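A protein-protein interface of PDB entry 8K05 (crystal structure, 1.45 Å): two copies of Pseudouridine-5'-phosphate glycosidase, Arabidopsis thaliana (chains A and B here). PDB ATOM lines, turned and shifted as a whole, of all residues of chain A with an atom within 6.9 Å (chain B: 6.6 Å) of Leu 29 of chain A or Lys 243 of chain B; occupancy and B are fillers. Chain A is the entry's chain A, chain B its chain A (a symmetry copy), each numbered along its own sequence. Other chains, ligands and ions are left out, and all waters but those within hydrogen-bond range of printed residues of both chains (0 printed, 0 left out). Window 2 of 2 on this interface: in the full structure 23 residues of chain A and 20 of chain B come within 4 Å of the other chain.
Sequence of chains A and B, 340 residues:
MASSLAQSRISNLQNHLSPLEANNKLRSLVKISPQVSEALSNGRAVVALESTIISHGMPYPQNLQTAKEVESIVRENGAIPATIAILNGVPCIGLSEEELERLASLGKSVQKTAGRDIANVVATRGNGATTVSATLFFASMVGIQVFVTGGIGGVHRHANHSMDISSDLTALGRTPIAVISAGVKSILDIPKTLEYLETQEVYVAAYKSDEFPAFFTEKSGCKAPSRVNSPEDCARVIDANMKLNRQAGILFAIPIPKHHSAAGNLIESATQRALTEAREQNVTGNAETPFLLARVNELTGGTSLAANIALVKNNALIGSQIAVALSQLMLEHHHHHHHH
OD2 of Asp 239 of chain B is in salt-bridge range of NZ of Lys 243 of chain B (3.4 Å).
Among the printed residues, merely in contact across the chains: Ile 118 of chain A with Leu 244 of chain B (3.6 Å), Leu 29 of chain A with Leu 244 of chain B (3.7 Å), Met 141 of chain A with Leu 244 of chain B (3.7 Å), Phe 138 of chain A with Leu 244 of chain B (3.8 Å), Val 122 of chain A with Ala 240 of chain B (3.9 Å) and Leu 29 of chain A with Lys 243 of chain B (3.996 Å).
Of the printed residues of chain A, Lys 243 of chain B touches Leu 29 (3.996 Å). Of the printed residues of chain A, Leu 244 of chain B touches Leu 29 (3.7 Å), Ile 118 (3.6 Å), Phe 138 (3.8 Å) and Met 141 (3.7 Å). Of the printed residues of chain B, Ile 118 of chain A touches Leu 244. Printed residues of chain B within 4 Å of Met 141 of chain A: Leu 244. Of the printed residues of chain B, Val 122 of chain A touches Ala 240 (3.9 Å). Leu 329 of chain B touches none of the printed residues of chain A. Lys 31 of chain A touches none of the printed residues of chain B. The nearest printed residue of chain B that does not touch Leu 29 of chain A is Ala 240 of chain B (4.5 Å). The nearest printed residue of chain B that does not touch Phe 138 of chain A is Arg 246 of chain B (6.8 Å).
Hydrophobic or aromatic side chains of chain A within 4 Å of the printed part of chain B: Leu 29, Ile 118, Val 122, Phe 138 and Met 141. Of the 11 printed residues of chain B, 3 touch a printed residue of chain A. Printed residues of chain B that touch a printed residue of chain A: Ala 240, Lys 243 and Leu 244. Hydrophobic or aromatic side chains of chain B within 4 Å of the printed part of chain A: Ala 240 and Leu 244. Among the printed residues, 6 pairs touch across the chains. Among the printed residues, no Asp or Glu carboxylate lies within 4 Å of a Lys or Arg side-chain nitrogen of the other chain.
No position is printed for both chains. Of the 6 pairs that touch across the chains among the printed residues, none has its exchanged pair printed and touching as well.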
ATOM      1  N   SER A  28     -12.643 -25.620  -2.001  1.00  0.00           N
ATOM      2  CA  SER A  28     -13.054 -26.353  -0.803  1.00  0.00           C
ATOM      3  C   SER A  28     -14.154 -25.615  -0.046  1.00  0.00           C
ATOM      4  O   SER A  28     -14.805 -26.176   0.840  1.00  0.00           O
ATOM      5  CB  SER A  28     -11.854 -26.589   0.118  1.00  0.00           C
ATOM      6  OG  SER A  28     -12.249 -27.259   1.304  1.00  0.00           O
ATOM      7  N   LEU A  29     -14.351 -24.351  -0.401  1.00  0.00           N
ATOM      8  CA  LEU A  29     -15.423 -23.541   0.157  1.00  0.00           C
ATOM      9  C   LEU A  29     -16.747 -23.911  -0.515  1.00  0.00           C
ATOM     10  O   LEU A  29     -17.806 -23.917   0.118  1.00  0.00           O
ATOM     11  CB  LEU A  29     -15.102 -22.054  -0.039  1.00  0.00           C
ATOM     12  CG  LEU A  29     -16.114 -20.958   0.281  1.00  0.00           C
ATOM     13  CD1 LEU A  29     -16.451 -20.929   1.765  1.00  0.00           C
ATOM     14  CD2 LEU A  29     -15.579 -19.598  -0.180  1.00  0.00           C
ATOM     15  N   VAL A  30     -16.666 -24.220  -1.804  1.00  0.00           N
ATOM     16  CA  VAL A  30     -17.842 -24.526  -2.609  1.00  0.00           C
ATOM     17  C   VAL A  30     -18.236 -25.995  -2.468  1.00  0.00           C
ATOM     18  O   VAL A  30     -17.394 -26.879  -2.584  1.00  0.00           O
ATOM     19  CB  VAL A  30     -17.590 -24.197  -4.098  1.00  0.00           C
ATOM     20  CG1 VAL A  30     -18.774 -24.609  -4.953  1.00  0.00           C
ATOM     21  CG2 VAL A  30     -17.301 -22.712  -4.270  1.00  0.00           C
ATOM     22  N   LYS A  31     -19.518 -26.248  -2.218  1.00  0.00           N
ATOM     23  CA  LYS A  31     -20.023 -27.612  -2.127  1.00  0.00           C
ATOM     24  C   LYS A  31     -20.718 -28.023  -3.420  1.00  0.00           C
ATOM     25  O   LYS A  31     -21.738 -27.444  -3.794  1.00  0.00           O
ATOM     26  CB  LYS A  31     -20.988 -27.749  -0.951  1.00  0.00           C
ATOM     27  CG  LYS A  31     -21.444 -29.183  -0.716  1.00  0.00           C
ATOM     28  CD  LYS A  31     -22.146 -29.334   0.620  1.00  0.00           C
ATOM     29  CE  LYS A  31     -23.463 -28.582   0.665  1.00  0.00           C
ATOM     30  NZ  LYS A  31     -24.498 -29.203  -0.215  1.00  0.00           N
ATOM     31  N   GLY A  89     -23.817 -19.319   4.201  1.00  0.00           N
ATOM     32  CA  GLY A  89     -22.470 -18.988   3.777  1.00  0.00           C
ATOM     33  C   GLY A  89     -21.781 -20.007   2.888  1.00  0.00           C
ATOM     34  O   GLY A  89     -20.627 -19.811   2.494  1.00  0.00           O
ATOM     35  N   VAL A  90     -22.468 -21.104   2.574  1.00  0.00           N
ATOM     36  CA  VAL A  90     -21.871 -22.147   1.755  1.00  0.00           C
ATOM     37  C   VAL A  90     -22.400 -22.083   0.336  1.00  0.00           C
ATOM     38  O   VAL A  90     -23.588 -22.305   0.115  1.00  0.00           O
ATOM     39  CB  VAL A  90     -22.152 -23.557   2.316  1.00  0.00           C
ATOM     40  CG1 VAL A  90     -21.469 -24.607   1.454  1.00  0.00           C
ATOM     41  CG2 VAL A  90     -21.690 -23.644   3.769  1.00  0.00           C
ATOM     42  N   PRO A  91     -21.529 -21.748  -0.636  1.00  0.00           N
ATOM     43  CA  PRO A  91     -21.982 -21.835  -2.025  1.00  0.00           C
ATOM     44  C   PRO A  91     -22.258 -23.283  -2.391  1.00  0.00           C
ATOM     45  O   PRO A  91     -21.383 -24.134  -2.248  1.00  0.00           O
ATOM     46  CB  PRO A  91     -20.802 -21.277  -2.833  1.00  0.00           C
ATOM     47  CG  PRO A  91     -19.959 -20.518  -1.830  1.00  0.00           C
ATOM     48  CD  PRO A  91     -20.138 -21.276  -0.533  1.00  0.00           C
ATOM     49  N   CYS A  92     -23.466 -23.537  -2.872  1.00  0.00           N
ATOM     50  CA  CYS A  92     -23.902 -24.872  -3.239  1.00  0.00           C
ATOM     51  C   CYS A  92     -24.168 -24.942  -4.722  1.00  0.00           C
ATOM     52  O   CYS A  92     -24.932 -24.148  -5.262  1.00  0.00           O
ATOM     53  CB  CYS A  92     -25.163 -25.255  -2.471  1.00  0.00           C
ATOM     54  SG  CYS A  92     -24.914 -25.415  -0.694  1.00  0.00           S
ATOM     55  N   ILE A 118     -21.043 -11.924  -3.471  1.00  0.00           N
ATOM     56  CA  ILE A 118     -20.801 -13.291  -3.015  1.00  0.00           C
ATOM     57  C   ILE A 118     -19.913 -13.342  -1.773  1.00  0.00           C
ATOM     58  O   ILE A 118     -20.262 -14.005  -0.792  1.00  0.00           O
ATOM     59  CB  ILE A 118     -20.158 -14.153  -4.118  1.00  0.00           C
ATOM     60  CG1 ILE A 118     -21.108 -14.262  -5.320  1.00  0.00           C
ATOM     61  CG2 ILE A 118     -19.790 -15.533  -3.566  1.00  0.00           C
ATOM     62  CD1 ILE A 118     -20.440 -14.849  -6.551  1.00  0.00           C
ATOM     63  N   VAL A 122     -20.923 -14.923   1.891  1.00  0.00           N
ATOM     64  CA  VAL A 122     -20.113 -15.980   2.494  1.00  0.00           C
ATOM     65  C   VAL A 122     -19.571 -15.544   3.860  1.00  0.00           C
ATOM     66  O   VAL A 122     -19.683 -16.285   4.849  1.00  0.00           O
ATOM     67  CB  VAL A 122     -18.952 -16.391   1.571  1.00  0.00           C
ATOM     68  CG1 VAL A 122     -17.951 -17.275   2.318  1.00  0.00           C
ATOM     69  CG2 VAL A 122     -19.501 -17.094   0.328  1.00  0.00           C
ATOM     70  N   PHE A 138     -20.057 -19.062 -10.509  1.00  0.00           N
ATOM     71  CA  PHE A 138     -19.945 -20.387  -9.902  1.00  0.00           C
ATOM     72  C   PHE A 138     -20.016 -21.513 -10.933  1.00  0.00           C
ATOM     73  O   PHE A 138     -19.286 -22.495 -10.845  1.00  0.00           O
ATOM     74  CB  PHE A 138     -21.036 -20.590  -8.853  1.00  0.00           C
ATOM     75  CG  PHE A 138     -20.747 -19.905  -7.548  1.00  0.00           C
ATOM     76  CD1 PHE A 138     -19.616 -20.238  -6.826  1.00  0.00           C
ATOM     77  CD2 PHE A 138     -21.607 -18.949  -7.047  1.00  0.00           C
ATOM     78  CE1 PHE A 138     -19.335 -19.609  -5.619  1.00  0.00           C
ATOM     79  CE2 PHE A 138     -21.341 -18.325  -5.835  1.00  0.00           C
ATOM     80  CZ  PHE A 138     -20.204 -18.656  -5.132  1.00  0.00           C
ATOM     81  N   MET A 141     -16.741 -21.686 -12.781  1.00  0.00           N
ATOM     82  CA  MET A 141     -15.699 -22.116 -11.843  1.00  0.00           C
ATOM     83  C   MET A 141     -15.522 -23.626 -11.860  1.00  0.00           C
ATOM     84  O   MET A 141     -14.406 -24.127 -11.786  1.00  0.00           O
ATOM     85  CB  MET A 141     -16.030 -21.662 -10.410  1.00  0.00           C
ATOM     86  CG  MET A 141     -15.117 -22.266  -9.331  1.00  0.00           C
ATOM     87  SD  MET A 141     -15.807 -22.237  -7.654  1.00  0.00           S
ATOM     88  CE  MET A 141     -15.779 -20.491  -7.292  1.00  0.00           C
ATOM     89  N   ILE B 238     -12.558 -10.017   2.655  1.00  0.00           N
ATOM     90  CA  ILE B 238     -11.353 -10.240   1.866  1.00  0.00           C
ATOM     91  C   ILE B 238     -10.984 -11.717   1.836  1.00  0.00           C
ATOM     92  O   ILE B 238     -10.673 -12.268   0.776  1.00  0.00           O
ATOM     93  CB  ILE B 238     -10.147  -9.425   2.401  1.00  0.00           C
ATOM     94  CG1 ILE B 238     -10.471  -7.928   2.331  1.00  0.00           C
ATOM     95  CG2 ILE B 238      -8.863  -9.771   1.643  1.00  0.00           C
ATOM     96  CD1 ILE B 238      -9.472  -7.069   3.100  1.00  0.00           C
ATOM     97  N   ASP B 239     -11.023 -12.363   3.000  1.00  0.00           N
ATOM     98  CA  ASP B 239     -10.710 -13.782   3.106  1.00  0.00           C
ATOM     99  C   ASP B 239     -11.631 -14.609   2.188  1.00  0.00           C
ATOM    100  O   ASP B 239     -11.155 -15.487   1.450  1.00  0.00           O
ATOM    101  CB  ASP B 239     -10.838 -14.212   4.582  1.00  0.00           C
ATOM    102  CG  ASP B 239     -10.524 -15.687   4.828  1.00  0.00           C
ATOM    103  OD1 ASP B 239      -9.457 -16.187   4.422  1.00  0.00           O
ATOM    104  OD2 ASP B 239     -11.374 -16.331   5.476  1.00  0.00           O
ATOM    105  N   ALA B 240     -12.925 -14.308   2.217  1.00  0.00           N
ATOM    106  CA  ALA B 240     -13.880 -15.006   1.349  1.00  0.00           C
ATOM    107  C   ALA B 240     -13.532 -14.762  -0.124  1.00  0.00           C
ATOM    108  O   ALA B 240     -13.498 -15.700  -0.931  1.00  0.00           O
ATOM    109  CB  ALA B 240     -15.293 -14.570   1.649  1.00  0.00           C
ATOM    110  N   ASN B 241     -13.226 -13.511  -0.463  1.00  0.00           N
ATOM    111  CA  ASN B 241     -12.880 -13.176  -1.839  1.00  0.00           C
ATOM    112  C   ASN B 241     -11.662 -13.951  -2.338  1.00  0.00           C
ATOM    113  O   ASN B 241     -11.635 -14.428  -3.487  1.00  0.00           O
ATOM    114  CB  ASN B 241     -12.644 -11.664  -1.967  1.00  0.00           C
ATOM    115  CG  ASN B 241     -12.919 -11.160  -3.374  1.00  0.00           C
ATOM    116  OD1 ASN B 241     -14.000 -11.409  -3.926  1.00  0.00           O
ATOM    117  ND2 ASN B 241     -11.960 -10.442  -3.956  1.00  0.00           N
ATOM    118  N   MET B 242     -10.650 -14.084  -1.481  1.00  0.00           N
ATOM    119  CA  MET B 242      -9.456 -14.863  -1.791  1.00  0.00           C
ATOM    120  C   MET B 242      -9.792 -16.341  -2.000  1.00  0.00           C
ATOM    121  O   MET B 242      -9.342 -16.947  -2.965  1.00  0.00           O
ATOM    122  CB  MET B 242      -8.415 -14.721  -0.673  1.00  0.00           C
ATOM    123  CG  MET B 242      -7.846 -13.313  -0.537  1.00  0.00           C
ATOM    124  SD  MET B 242      -6.790 -13.188   0.935  1.00  0.00           S
ATOM    125  CE  MET B 242      -5.405 -14.196   0.460  1.00  0.00           C
ATOM    126  N   LYS B 243     -10.570 -16.915  -1.086  1.00  0.00           N
ATOM    127  CA  LYS B 243     -10.894 -18.344  -1.158  1.00  0.00           C
ATOM    128  C   LYS B 243     -11.702 -18.662  -2.404  1.00  0.00           C
ATOM    129  O   LYS B 243     -11.555 -19.740  -2.987  1.00  0.00           O
ATOM    130  CB  LYS B 243     -11.674 -18.787   0.073  1.00  0.00           C
ATOM    131  CG  LYS B 243     -10.889 -18.766   1.364  1.00  0.00           C
ATOM    132  CD  LYS B 243     -11.866 -18.680   2.527  1.00  0.00           C
ATOM    133  CE  LYS B 243     -11.389 -19.417   3.754  1.00  0.00           C
ATOM    134  NZ  LYS B 243     -12.511 -19.503   4.739  1.00  0.00           N
ATOM    135  N   LEU B 244     -12.560 -17.726  -2.796  1.00  0.00           N
ATOM    136  CA  LEU B 244     -13.382 -17.887  -3.991  1.00  0.00           C
ATOM    137  C   LEU B 244     -12.601 -17.743  -5.291  1.00  0.00           C
ATOM    138  O   LEU B 244     -13.116 -18.099  -6.355  1.00  0.00           O
ATOM    139  CB  LEU B 244     -14.517 -16.874  -3.983  1.00  0.00           C
ATOM    140  CG  LEU B 244     -15.604 -17.041  -2.932  1.00  0.00           C
ATOM    141  CD1 LEU B 244     -16.346 -15.734  -2.720  1.00  0.00           C
ATOM    142  CD2 LEU B 244     -16.572 -18.128  -3.392  1.00  0.00           C
ATOM    143  N   ASN B 245     -11.382 -17.207  -5.211  1.00  0.00           N
ATOM    144  CA  ASN B 245     -10.560 -16.888  -6.376  1.00  0.00           C
ATOM    145  C   ASN B 245     -11.257 -15.937  -7.356  1.00  0.00           C
ATOM    146  O   ASN B 245     -11.040 -16.019  -8.573  1.00  0.00           O
ATOM    147  CB  ASN B 245     -10.127 -18.177  -7.103  1.00  0.00           C
ATOM    148  CG  ASN B 245      -8.935 -17.960  -8.011  1.00  0.00           C
ATOM    149  OD1 ASN B 245      -8.014 -17.205  -7.686  1.00  0.00           O
ATOM    150  ND2 ASN B 245      -8.943 -18.624  -9.164  1.00  0.00           N
ATOM    151  N   ARG B 246     -12.070 -15.019  -6.831  1.00  0.00           N
ATOM    152  CA  ARG B 246     -12.682 -13.971  -7.653  1.00  0.00           C
ATOM    153  C   ARG B 246     -11.602 -13.043  -8.182  1.00  0.00           C
ATOM    154  O   ARG B 246     -10.640 -12.753  -7.478  1.00  0.00           O
ATOM    155  CB  ARG B 246     -13.693 -13.142  -6.857  1.00  0.00           C
ATOM    156  CG  ARG B 246     -14.922 -13.879  -6.362  1.00  0.00           C
ATOM    157  CD  ARG B 246     -16.150 -13.655  -7.253  1.00  0.00           C
ATOM    158  NE  ARG B 246     -16.539 -12.256  -7.489  1.00  0.00           N
ATOM    159  CZ  ARG B 246     -17.297 -11.867  -8.523  1.00  0.00           C
ATOM    160  NH1 ARG B 246     -17.600 -10.582  -8.674  1.00  0.00           N
ATOM    161  NH2 ARG B 246     -17.757 -12.759  -9.417  1.00  0.00           N
ATOM    162  N   LEU B 329      -6.911 -14.729  10.052  1.00  0.00           N
ATOM    163  CA  LEU B 329      -7.776 -15.656   9.327  1.00  0.00           C
ATOM    164  C   LEU B 329      -6.948 -16.601   8.474  1.00  0.00           C
ATOM    165  O   LEU B 329      -7.240 -17.799   8.398  1.00  0.00           O
ATOM    166  CB  LEU B 329      -8.783 -14.892   8.456  1.00  0.00           C
ATOM    167  CG  LEU B 329      -9.857 -14.132   9.224  1.00  0.00           C
ATOM    168  CD1 LEU B 329     -10.743 -13.327   8.275  1.00  0.00           C
ATOM    169  CD2 LEU B 329     -10.699 -15.101  10.056  1.00  0.00           C
ATOM    170  N   HIS B 333      -6.408 -20.990   8.736  1.00  0.00           N
ATOM    171  CA  HIS B 333      -6.873 -21.864   7.659  1.00  0.00           C
ATOM    172  C   HIS B 333      -6.476 -23.311   7.934  1.00  0.00           C
ATOM    173  O   HIS B 333      -5.402 -23.565   8.474  1.00  0.00           O
ATOM    174  CB  HIS B 333      -6.308 -21.423   6.308  1.00  0.00           C
ATOM    175  CG  HIS B 333      -6.987 -20.220   5.730  1.00  0.00           C
ATOM    176  ND1 HIS B 333      -6.436 -19.476   4.708  1.00  0.00           N
ATOM    177  CD2 HIS B 333      -8.173 -19.637   6.024  1.00  0.00           C
ATOM    178  CE1 HIS B 333      -7.252 -18.483   4.402  1.00  0.00           C
ATOM    179  NE2 HIS B 333      -8.312 -18.555   5.188  1.00  0.00           N
